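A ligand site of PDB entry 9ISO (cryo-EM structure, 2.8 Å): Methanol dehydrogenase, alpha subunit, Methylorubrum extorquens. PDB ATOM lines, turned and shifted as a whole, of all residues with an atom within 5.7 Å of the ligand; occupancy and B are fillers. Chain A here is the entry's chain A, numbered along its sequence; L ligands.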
ATOM      1  N   GLU A  82     -19.229 -27.603 -30.206  1.00  0.00           N
ATOM      2  CA  GLU A  82     -18.142 -26.936 -30.909  1.00  0.00           C
ATOM      3  C   GLU A  82     -17.487 -27.911 -31.884  1.00  0.00           C
ATOM      4  O   GLU A  82     -17.615 -29.138 -31.759  1.00  0.00           O
ATOM      5  CB  GLU A  82     -17.102 -26.386 -29.940  1.00  0.00           C
ATOM      6  CG  GLU A  82     -17.448 -25.025 -29.360  1.00  0.00           C
ATOM      7  CD  GLU A  82     -16.530 -24.623 -28.231  1.00  0.00           C
ATOM      8  OE1 GLU A  82     -16.968 -23.826 -27.356  1.00  0.00           O
ATOM      9  OE2 GLU A  82     -15.379 -25.102 -28.191  1.00  0.00           O
ATOM     10  N   CYS A 130     -13.967 -24.981 -16.463  1.00  0.00           N
ATOM     11  CA  CYS A 130     -13.956 -23.536 -16.265  1.00  0.00           C
ATOM     12  C   CYS A 130     -15.290 -22.912 -16.618  1.00  0.00           C
ATOM     13  O   CYS A 130     -15.887 -22.181 -15.819  1.00  0.00           O
ATOM     14  CB  CYS A 130     -12.863 -22.894 -17.132  1.00  0.00           C
ATOM     15  SG  CYS A 130     -13.316 -22.781 -18.905  1.00  0.00           S
ATOM     16  N   CYS A 131     -15.778 -23.182 -17.824  1.00  0.00           N
ATOM     17  CA  CYS A 131     -16.736 -22.292 -18.456  1.00  0.00           C
ATOM     18  C   CYS A 131     -17.972 -23.032 -18.958  1.00  0.00           C
ATOM     19  O   CYS A 131     -19.087 -22.522 -18.854  1.00  0.00           O
ATOM     20  CB  CYS A 131     -16.034 -21.545 -19.590  1.00  0.00           C
ATOM     21  SG  CYS A 131     -14.337 -21.040 -19.138  1.00  0.00           S
ATOM     22  N   ASP A 132     -17.779 -24.234 -19.489  1.00  0.00           N
ATOM     23  CA  ASP A 132     -18.851 -25.055 -20.038  1.00  0.00           C
ATOM     24  C   ASP A 132     -18.259 -26.402 -20.417  1.00  0.00           C
ATOM     25  O   ASP A 132     -17.033 -26.548 -20.554  1.00  0.00           O
ATOM     26  CB  ASP A 132     -19.509 -24.395 -21.254  1.00  0.00           C
ATOM     27  CG  ASP A 132     -20.900 -24.909 -21.514  1.00  0.00           C
ATOM     28  OD1 ASP A 132     -21.527 -25.439 -20.569  1.00  0.00           O
ATOM     29  OD2 ASP A 132     -21.383 -24.776 -22.656  1.00  0.00           O
ATOM     30  N   VAL A 134     -17.430 -28.709 -23.057  1.00  0.00           N
ATOM     31  CA  VAL A 134     -17.245 -28.606 -24.493  1.00  0.00           C
ATOM     32  C   VAL A 134     -16.138 -29.558 -24.942  1.00  0.00           C
ATOM     33  O   VAL A 134     -15.337 -30.050 -24.151  1.00  0.00           O
ATOM     34  CB  VAL A 134     -16.916 -27.167 -24.936  1.00  0.00           C
ATOM     35  CG1 VAL A 134     -18.121 -26.272 -24.767  1.00  0.00           C
ATOM     36  CG2 VAL A 134     -15.742 -26.623 -24.140  1.00  0.00           C
ATOM     37  N   ARG A 136     -13.752 -30.273 -28.925  1.00  0.00           N
ATOM     38  CA  ARG A 136     -13.385 -29.581 -30.150  1.00  0.00           C
ATOM     39  C   ARG A 136     -12.949 -30.509 -31.281  1.00  0.00           C
ATOM     40  O   ARG A 136     -12.262 -30.049 -32.202  1.00  0.00           O
ATOM     41  CB  ARG A 136     -12.294 -28.548 -29.870  1.00  0.00           C
ATOM     42  CG  ARG A 136     -12.804 -27.298 -29.174  1.00  0.00           C
ATOM     43  CD  ARG A 136     -11.711 -26.257 -29.020  1.00  0.00           C
ATOM     44  NE  ARG A 136     -12.194 -25.083 -28.303  1.00  0.00           N
ATOM     45  CZ  ARG A 136     -12.083 -24.910 -26.996  1.00  0.00           C
ATOM     46  NH1 ARG A 136     -11.494 -25.806 -26.227  1.00  0.00           N
ATOM     47  NH2 ARG A 136     -12.580 -23.806 -26.447  1.00  0.00           N
ATOM     48  N   THR A 186     -10.104 -30.639 -22.916  1.00  0.00           N
ATOM     49  CA  THR A 186     -11.179 -30.373 -23.867  1.00  0.00           C
ATOM     50  C   THR A 186     -10.665 -30.066 -25.267  1.00  0.00           C
ATOM     51  O   THR A 186     -11.451 -29.631 -26.114  1.00  0.00           O
ATOM     52  CB  THR A 186     -12.053 -29.215 -23.377  1.00  0.00           C
ATOM     53  OG1 THR A 186     -11.266 -28.022 -23.272  1.00  0.00           O
ATOM     54  CG2 THR A 186     -12.670 -29.539 -22.028  1.00  0.00           C
ATOM     55  N   SER A 201      -5.476 -28.326 -20.194  1.00  0.00           N
ATOM     56  CA  SER A 201      -6.233 -27.127 -19.874  1.00  0.00           C
ATOM     57  C   SER A 201      -6.491 -27.079 -18.369  1.00  0.00           C
ATOM     58  O   SER A 201      -6.364 -28.088 -17.669  1.00  0.00           O
ATOM     59  CB  SER A 201      -7.554 -27.053 -20.640  1.00  0.00           C
ATOM     60  OG  SER A 201      -8.428 -28.091 -20.252  1.00  0.00           O
ATOM     61  N   GLY A 202      -6.865 -25.904 -17.890  1.00  0.00           N
ATOM     62  CA  GLY A 202      -7.150 -25.704 -16.486  1.00  0.00           C
ATOM     63  C   GLY A 202      -6.243 -24.702 -15.796  1.00  0.00           C
ATOM     64  O   GLY A 202      -5.951 -24.842 -14.606  1.00  0.00           O
ATOM     65  N   ALA A 203      -5.791 -23.694 -16.531  1.00  0.00           N
ATOM     66  CA  ALA A 203      -4.844 -22.731 -15.975  1.00  0.00           C
ATOM     67  C   ALA A 203      -5.468 -21.824 -14.926  1.00  0.00           C
ATOM     68  O   ALA A 203      -4.736 -21.206 -14.148  1.00  0.00           O
ATOM     69  CB  ALA A 203      -4.236 -21.886 -17.097  1.00  0.00           C
ATOM     70  N   GLU A 204      -6.803 -21.718 -14.894  1.00  0.00           N
ATOM     71  CA  GLU A 204      -7.446 -20.851 -13.900  1.00  0.00           C
ATOM     72  C   GLU A 204      -7.241 -21.371 -12.486  1.00  0.00           C
ATOM     73  O   GLU A 204      -7.274 -20.595 -11.532  1.00  0.00           O
ATOM     74  CB  GLU A 204      -8.926 -20.708 -14.222  1.00  0.00           C
ATOM     75  CG  GLU A 204      -9.675 -19.718 -13.345  1.00  0.00           C
ATOM     76  CD  GLU A 204     -11.175 -19.811 -13.508  1.00  0.00           C
ATOM     77  OE1 GLU A 204     -11.639 -20.494 -14.452  1.00  0.00           O
ATOM     78  OE2 GLU A 204     -11.904 -19.208 -12.699  1.00  0.00           O
ATOM     79  N   THR A 268      -1.229 -23.088 -20.116  1.00  0.00           N
ATOM     80  CA  THR A 268      -1.784 -24.245 -20.780  1.00  0.00           C
ATOM     81  C   THR A 268      -2.276 -23.872 -22.178  1.00  0.00           C
ATOM     82  O   THR A 268      -2.788 -22.767 -22.402  1.00  0.00           O
ATOM     83  CB  THR A 268      -2.935 -24.843 -19.963  1.00  0.00           C
ATOM     84  OG1 THR A 268      -4.019 -23.906 -19.923  1.00  0.00           O
ATOM     85  CG2 THR A 268      -2.477 -25.142 -18.553  1.00  0.00           C
ATOM     86  N   TRP A 270      -4.819 -24.803 -25.296  1.00  0.00           N
ATOM     87  CA  TRP A 270      -6.074 -25.488 -25.604  1.00  0.00           C
ATOM     88  C   TRP A 270      -6.655 -25.012 -26.927  1.00  0.00           C
ATOM     89  O   TRP A 270      -7.871 -24.992 -27.111  1.00  0.00           O
ATOM     90  CB  TRP A 270      -7.094 -25.279 -24.489  1.00  0.00           C
ATOM     91  CG  TRP A 270      -7.203 -23.860 -23.991  1.00  0.00           C
ATOM     92  CD1 TRP A 270      -6.399 -23.266 -23.058  1.00  0.00           C
ATOM     93  CD2 TRP A 270      -8.148 -22.868 -24.408  1.00  0.00           C
ATOM     94  NE1 TRP A 270      -6.799 -21.961 -22.864  1.00  0.00           N
ATOM     95  CE2 TRP A 270      -7.865 -21.698 -23.681  1.00  0.00           C
ATOM     96  CE3 TRP A 270      -9.209 -22.861 -25.317  1.00  0.00           C
ATOM     97  CZ2 TRP A 270      -8.599 -20.528 -23.835  1.00  0.00           C
ATOM     98  CZ3 TRP A 270      -9.938 -21.699 -25.474  1.00  0.00           C
ATOM     99  CH2 TRP A 270      -9.627 -20.552 -24.738  1.00  0.00           C
ATOM    100  N   ASN A 288      -2.395 -17.966 -20.468  1.00  0.00           N
ATOM    101  CA  ASN A 288      -2.076 -16.947 -19.485  1.00  0.00           C
ATOM    102  C   ASN A 288      -1.454 -17.537 -18.215  1.00  0.00           C
ATOM    103  O   ASN A 288      -1.599 -18.739 -17.943  1.00  0.00           O
ATOM    104  CB  ASN A 288      -3.338 -16.148 -19.131  1.00  0.00           C
ATOM    105  CG  ASN A 288      -4.429 -16.996 -18.503  1.00  0.00           C
ATOM    106  OD1 ASN A 288      -4.238 -18.179 -18.210  1.00  0.00           O
ATOM    107  ND2 ASN A 288      -5.600 -16.394 -18.304  1.00  0.00           N
ATOM    108  N   ALA A 332      -5.321 -14.381 -23.374  1.00  0.00           N
ATOM    109  CA  ALA A 332      -4.907 -15.762 -23.639  1.00  0.00           C
ATOM    110  C   ALA A 332      -4.566 -15.894 -25.109  1.00  0.00           C
ATOM    111  O   ALA A 332      -5.436 -15.745 -25.967  1.00  0.00           O
ATOM    112  CB  ALA A 332      -6.019 -16.744 -23.253  1.00  0.00           C
ATOM    113  N   ARG A 358      -6.001 -11.940 -28.607  1.00  0.00           N
ATOM    114  CA  ARG A 358      -7.073 -11.379 -27.800  1.00  0.00           C
ATOM    115  C   ARG A 358      -6.828  -9.933 -27.379  1.00  0.00           C
ATOM    116  O   ARG A 358      -7.751  -9.296 -26.860  1.00  0.00           O
ATOM    117  CB  ARG A 358      -7.288 -12.232 -26.551  1.00  0.00           C
ATOM    118  CG  ARG A 358      -7.749 -13.644 -26.836  1.00  0.00           C
ATOM    119  CD  ARG A 358      -8.949 -14.020 -25.975  1.00  0.00           C
ATOM    120  NE  ARG A 358      -8.564 -14.509 -24.665  1.00  0.00           N
ATOM    121  CZ  ARG A 358      -9.410 -14.738 -23.669  1.00  0.00           C
ATOM    122  NH1 ARG A 358     -10.706 -14.505 -23.802  1.00  0.00           N
ATOM    123  NH2 ARG A 358      -8.944 -15.200 -22.512  1.00  0.00           N
ATOM    124  N   ALA A 416     -11.757  -8.665 -21.325  1.00  0.00           N
ATOM    125  CA  ALA A 416     -11.104  -9.960 -21.121  1.00  0.00           C
ATOM    126  C   ALA A 416     -11.518 -10.975 -22.173  1.00  0.00           C
ATOM    127  O   ALA A 416     -10.756 -11.897 -22.484  1.00  0.00           O
ATOM    128  CB  ALA A 416     -11.415 -10.474 -19.720  1.00  0.00           C
ATOM    129  N   ASN A 421     -11.450 -15.183 -30.251  1.00  0.00           N
ATOM    130  CA  ASN A 421     -11.440 -16.346 -29.371  1.00  0.00           C
ATOM    131  C   ASN A 421     -11.322 -17.597 -30.239  1.00  0.00           C
ATOM    132  O   ASN A 421     -10.878 -17.539 -31.384  1.00  0.00           O
ATOM    133  CB  ASN A 421     -12.666 -16.346 -28.453  1.00  0.00           C
ATOM    134  CG  ASN A 421     -12.365 -16.958 -27.103  1.00  0.00           C
ATOM    135  OD1 ASN A 421     -11.637 -17.942 -27.007  1.00  0.00           O
ATOM    136  ND2 ASN A 421     -12.890 -16.358 -26.043  1.00  0.00           N
ATOM    137  N   GLN A 422     -11.712 -18.741 -29.671  1.00  0.00           N
ATOM    138  CA  GLN A 422     -11.367 -20.066 -30.181  1.00  0.00           C
ATOM    139  C   GLN A 422     -11.914 -20.395 -31.562  1.00  0.00           C
ATOM    140  O   GLN A 422     -11.789 -21.529 -32.020  1.00  0.00           O
ATOM    141  CB  GLN A 422     -11.833 -21.125 -29.179  1.00  0.00           C
ATOM    142  CG  GLN A 422     -13.230 -20.881 -28.632  1.00  0.00           C
ATOM    143  CD  GLN A 422     -14.301 -21.574 -29.451  1.00  0.00           C
ATOM    144  OE1 GLN A 422     -14.081 -22.654 -30.008  1.00  0.00           O
ATOM    145  NE2 GLN A 422     -15.467 -20.953 -29.544  1.00  0.00           N
ATOM    146  N   TRP A 503     -18.996 -15.836 -32.170  1.00  0.00           N
ATOM    147  CA  TRP A 503     -18.299 -16.844 -31.388  1.00  0.00           C
ATOM    148  C   TRP A 503     -18.225 -18.100 -32.244  1.00  0.00           C
ATOM    149  O   TRP A 503     -19.113 -18.951 -32.217  1.00  0.00           O
ATOM    150  CB  TRP A 503     -19.019 -17.108 -30.073  1.00  0.00           C
ATOM    151  CG  TRP A 503     -18.115 -17.398 -28.924  1.00  0.00           C
ATOM    152  CD1 TRP A 503     -17.779 -18.620 -28.446  1.00  0.00           C
ATOM    153  CD2 TRP A 503     -17.455 -16.444 -28.085  1.00  0.00           C
ATOM    154  NE1 TRP A 503     -16.941 -18.500 -27.370  1.00  0.00           N
ATOM    155  CE2 TRP A 503     -16.732 -17.170 -27.130  1.00  0.00           C
ATOM    156  CE3 TRP A 503     -17.411 -15.052 -28.063  1.00  0.00           C
ATOM    157  CZ2 TRP A 503     -15.966 -16.542 -26.149  1.00  0.00           C
ATOM    158  CZ3 TRP A 503     -16.651 -14.435 -27.093  1.00  0.00           C
ATOM    159  CH2 TRP A 503     -15.935 -15.173 -26.149  1.00  0.00           C
ATOM    160  N   GLY A 566     -20.992 -22.208 -24.213  1.00  0.00           N
ATOM    161  CA  GLY A 566     -19.775 -21.432 -24.099  1.00  0.00           C
ATOM    162  C   GLY A 566     -19.897 -20.308 -23.076  1.00  0.00           C
ATOM    163  O   GLY A 566     -20.810 -20.246 -22.270  1.00  0.00           O
ATOM    164  N   TRP A 567     -18.919 -19.402 -23.149  1.00  0.00           N
ATOM    165  CA  TRP A 567     -18.912 -18.246 -22.248  1.00  0.00           C
ATOM    166  C   TRP A 567     -20.139 -17.361 -22.443  1.00  0.00           C
ATOM    167  O   TRP A 567     -20.786 -17.033 -21.434  1.00  0.00           O
ATOM    168  CB  TRP A 567     -17.607 -17.471 -22.441  1.00  0.00           C
ATOM    169  CG  TRP A 567     -17.319 -16.423 -21.381  1.00  0.00           C
ATOM    170  CD1 TRP A 567     -18.214 -15.849 -20.524  1.00  0.00           C
ATOM    171  CD2 TRP A 567     -16.053 -15.819 -21.103  1.00  0.00           C
ATOM    172  NE1 TRP A 567     -17.580 -14.936 -19.718  1.00  0.00           N
ATOM    173  CE2 TRP A 567     -16.259 -14.898 -20.054  1.00  0.00           C
ATOM    174  CE3 TRP A 567     -14.765 -15.963 -21.634  1.00  0.00           C
ATOM    175  CZ2 TRP A 567     -15.220 -14.125 -19.527  1.00  0.00           C
ATOM    176  CZ3 TRP A 567     -13.742 -15.200 -21.104  1.00  0.00           C
ATOM    177  CH2 TRP A 567     -13.976 -14.293 -20.062  1.00  0.00           C
ATOM    178  N   PRO A 568     -20.511 -16.947 -23.654  1.00  0.00           N
ATOM    179  CA  PRO A 568     -21.708 -16.092 -23.779  1.00  0.00           C
ATOM    180  C   PRO A 568     -22.993 -16.771 -23.342  1.00  0.00           C
ATOM    181  O   PRO A 568     -23.945 -16.079 -22.962  1.00  0.00           O
ATOM    182  CB  PRO A 568     -21.734 -15.743 -25.271  1.00  0.00           C
ATOM    183  CG  PRO A 568     -20.950 -16.814 -25.921  1.00  0.00           C
ATOM    184  CD  PRO A 568     -19.862 -17.136 -24.962  1.00  0.00           C
HETATM  185  N1  LIG L   1     -13.227 -21.468 -22.881  1.00  0.00           N
HETATM  186  C1  LIG L   1     -14.086 -20.630 -23.549  1.00  0.00           C
HETATM  187  C2  LIG L   1     -15.269 -21.095 -24.306  1.00  0.00           C
HETATM  188  O1  LIG L   1     -15.503 -22.330 -24.301  1.00  0.00           O
HETATM  189  O2  LIG L   1     -15.964 -20.236 -24.897  1.00  0.00           O
HETATM  190  C3  LIG L   1     -13.642 -19.311 -23.372  1.00  0.00           C
HETATM  191  C4  LIG L   1     -12.500 -19.362 -22.586  1.00  0.00           C
HETATM  192  C5  LIG L   1     -12.246 -20.718 -22.280  1.00  0.00           C
HETATM  193  C6  LIG L   1     -11.628 -18.311 -22.099  1.00  0.00           C
HETATM  194  O3  LIG L   1     -11.696 -17.141 -22.426  1.00  0.00           O
HETATM  195  C7  LIG L   1     -10.527 -18.739 -21.091  1.00  0.00           C
HETATM  196  O4  LIG L   1      -9.899 -17.864 -20.500  1.00  0.00           O
HETATM  197  C8  LIG L   1     -10.263 -20.189 -20.878  1.00  0.00           C
HETATM  198  N2  LIG L   1      -9.208 -20.507 -20.131  1.00  0.00           N
HETATM  199  C9  LIG L   1      -8.934 -21.805 -19.924  1.00  0.00           C
HETATM  200  C10 LIG L   1      -7.728 -22.131 -19.071  1.00  0.00           C
HETATM  201  O5  LIG L   1      -7.485 -23.340 -18.860  1.00  0.00           O
HETATM  202  O6  LIG L   1      -7.063 -21.165 -18.651  1.00  0.00           O
HETATM  203  C11 LIG L   1      -9.709 -22.831 -20.463  1.00  0.00           C
HETATM  204  C12 LIG L   1     -10.803 -22.513 -21.242  1.00  0.00           C
HETATM  205  C13 LIG L   1     -11.592 -23.690 -21.786  1.00  0.00           C
HETATM  206  O7  LIG L   1     -12.621 -23.512 -22.471  1.00  0.00           O
HETATM  207  O8  LIG L   1     -11.157 -24.827 -21.495  1.00  0.00           O
HETATM  208  C14 LIG L   1     -11.122 -21.150 -21.468  1.00  0.00           C
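An oxygen (O7) of the ligand sits close to the side-chain sulfur of Cys 130 (3.7 Å).
OE1 of Glu 82 touches O1 of the ligand (3.7 Å).
Cys 131 touches the ligand (SG to C5, 3.8 Å).
Thr 186 touches the ligand (OG1 to O8, 3.7 Å).
Ser 201 touches the ligand (C to O5, 3.9 Å).
Glu 204 touches the ligand.
OG1 of Thr 268 touches O5 of the ligand, 3.7 Å away.
Trp 270 touches the ligand (CZ2 to C8, 3.4 Å).
ND2 of Asn 421 touches O3 of the ligand, 3.9 Å away.
Trp 567 touches the ligand.
Hydrophobic or aromatic side chains within 4 Å of the ligand: Ala 203, Trp 270, Trp 503 and Trp 567.
Within 4 Å of the ligand: Glu 82, Cys 130, Cys 131, Arg 136, Thr 186, Ser 201, Gly 202, Ala 203, Glu 204, Thr 268, Trp 270, Arg 358, Asn 421, Trp 503 and Trp 567.
O of Ala 416 lies within hydrogen-bond range of NH1 of Arg 358 (2.9 Å).
SG of Cys 131 is disulfide-bonded to SG of Cys 130 (2.0 Å).
The side-chain carboxylate (OE2) of Glu 82 is in salt-bridge range of the guanidinium group (NE) of Arg 136.
OE1 of Gln 422 sits close to OE2 of Glu 82 (3.3 Å).
An oxygen (O5) of the ligand is in hydrogen-bond range of the backbone NH of Gly 202, at 2.8 Å.
The backbone NH (N) of Ala 203 is in hydrogen-bond range of an oxygen (O5) of the ligand, 2.9 Å away.
An oxygen (O3) of the ligand lies within hydrogen-bond range of the guanidinium group (NH1) of Arg 358 (3.1 Å).
An oxygen (O2) of the ligand sits at hydrogen-bond distance from the indole nitrogen (NE1) of Trp 503 (3.2 Å).
An oxygen (O1) of the ligand lies within salt-bridge range of the guanidinium group (NH2) of Arg 136.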
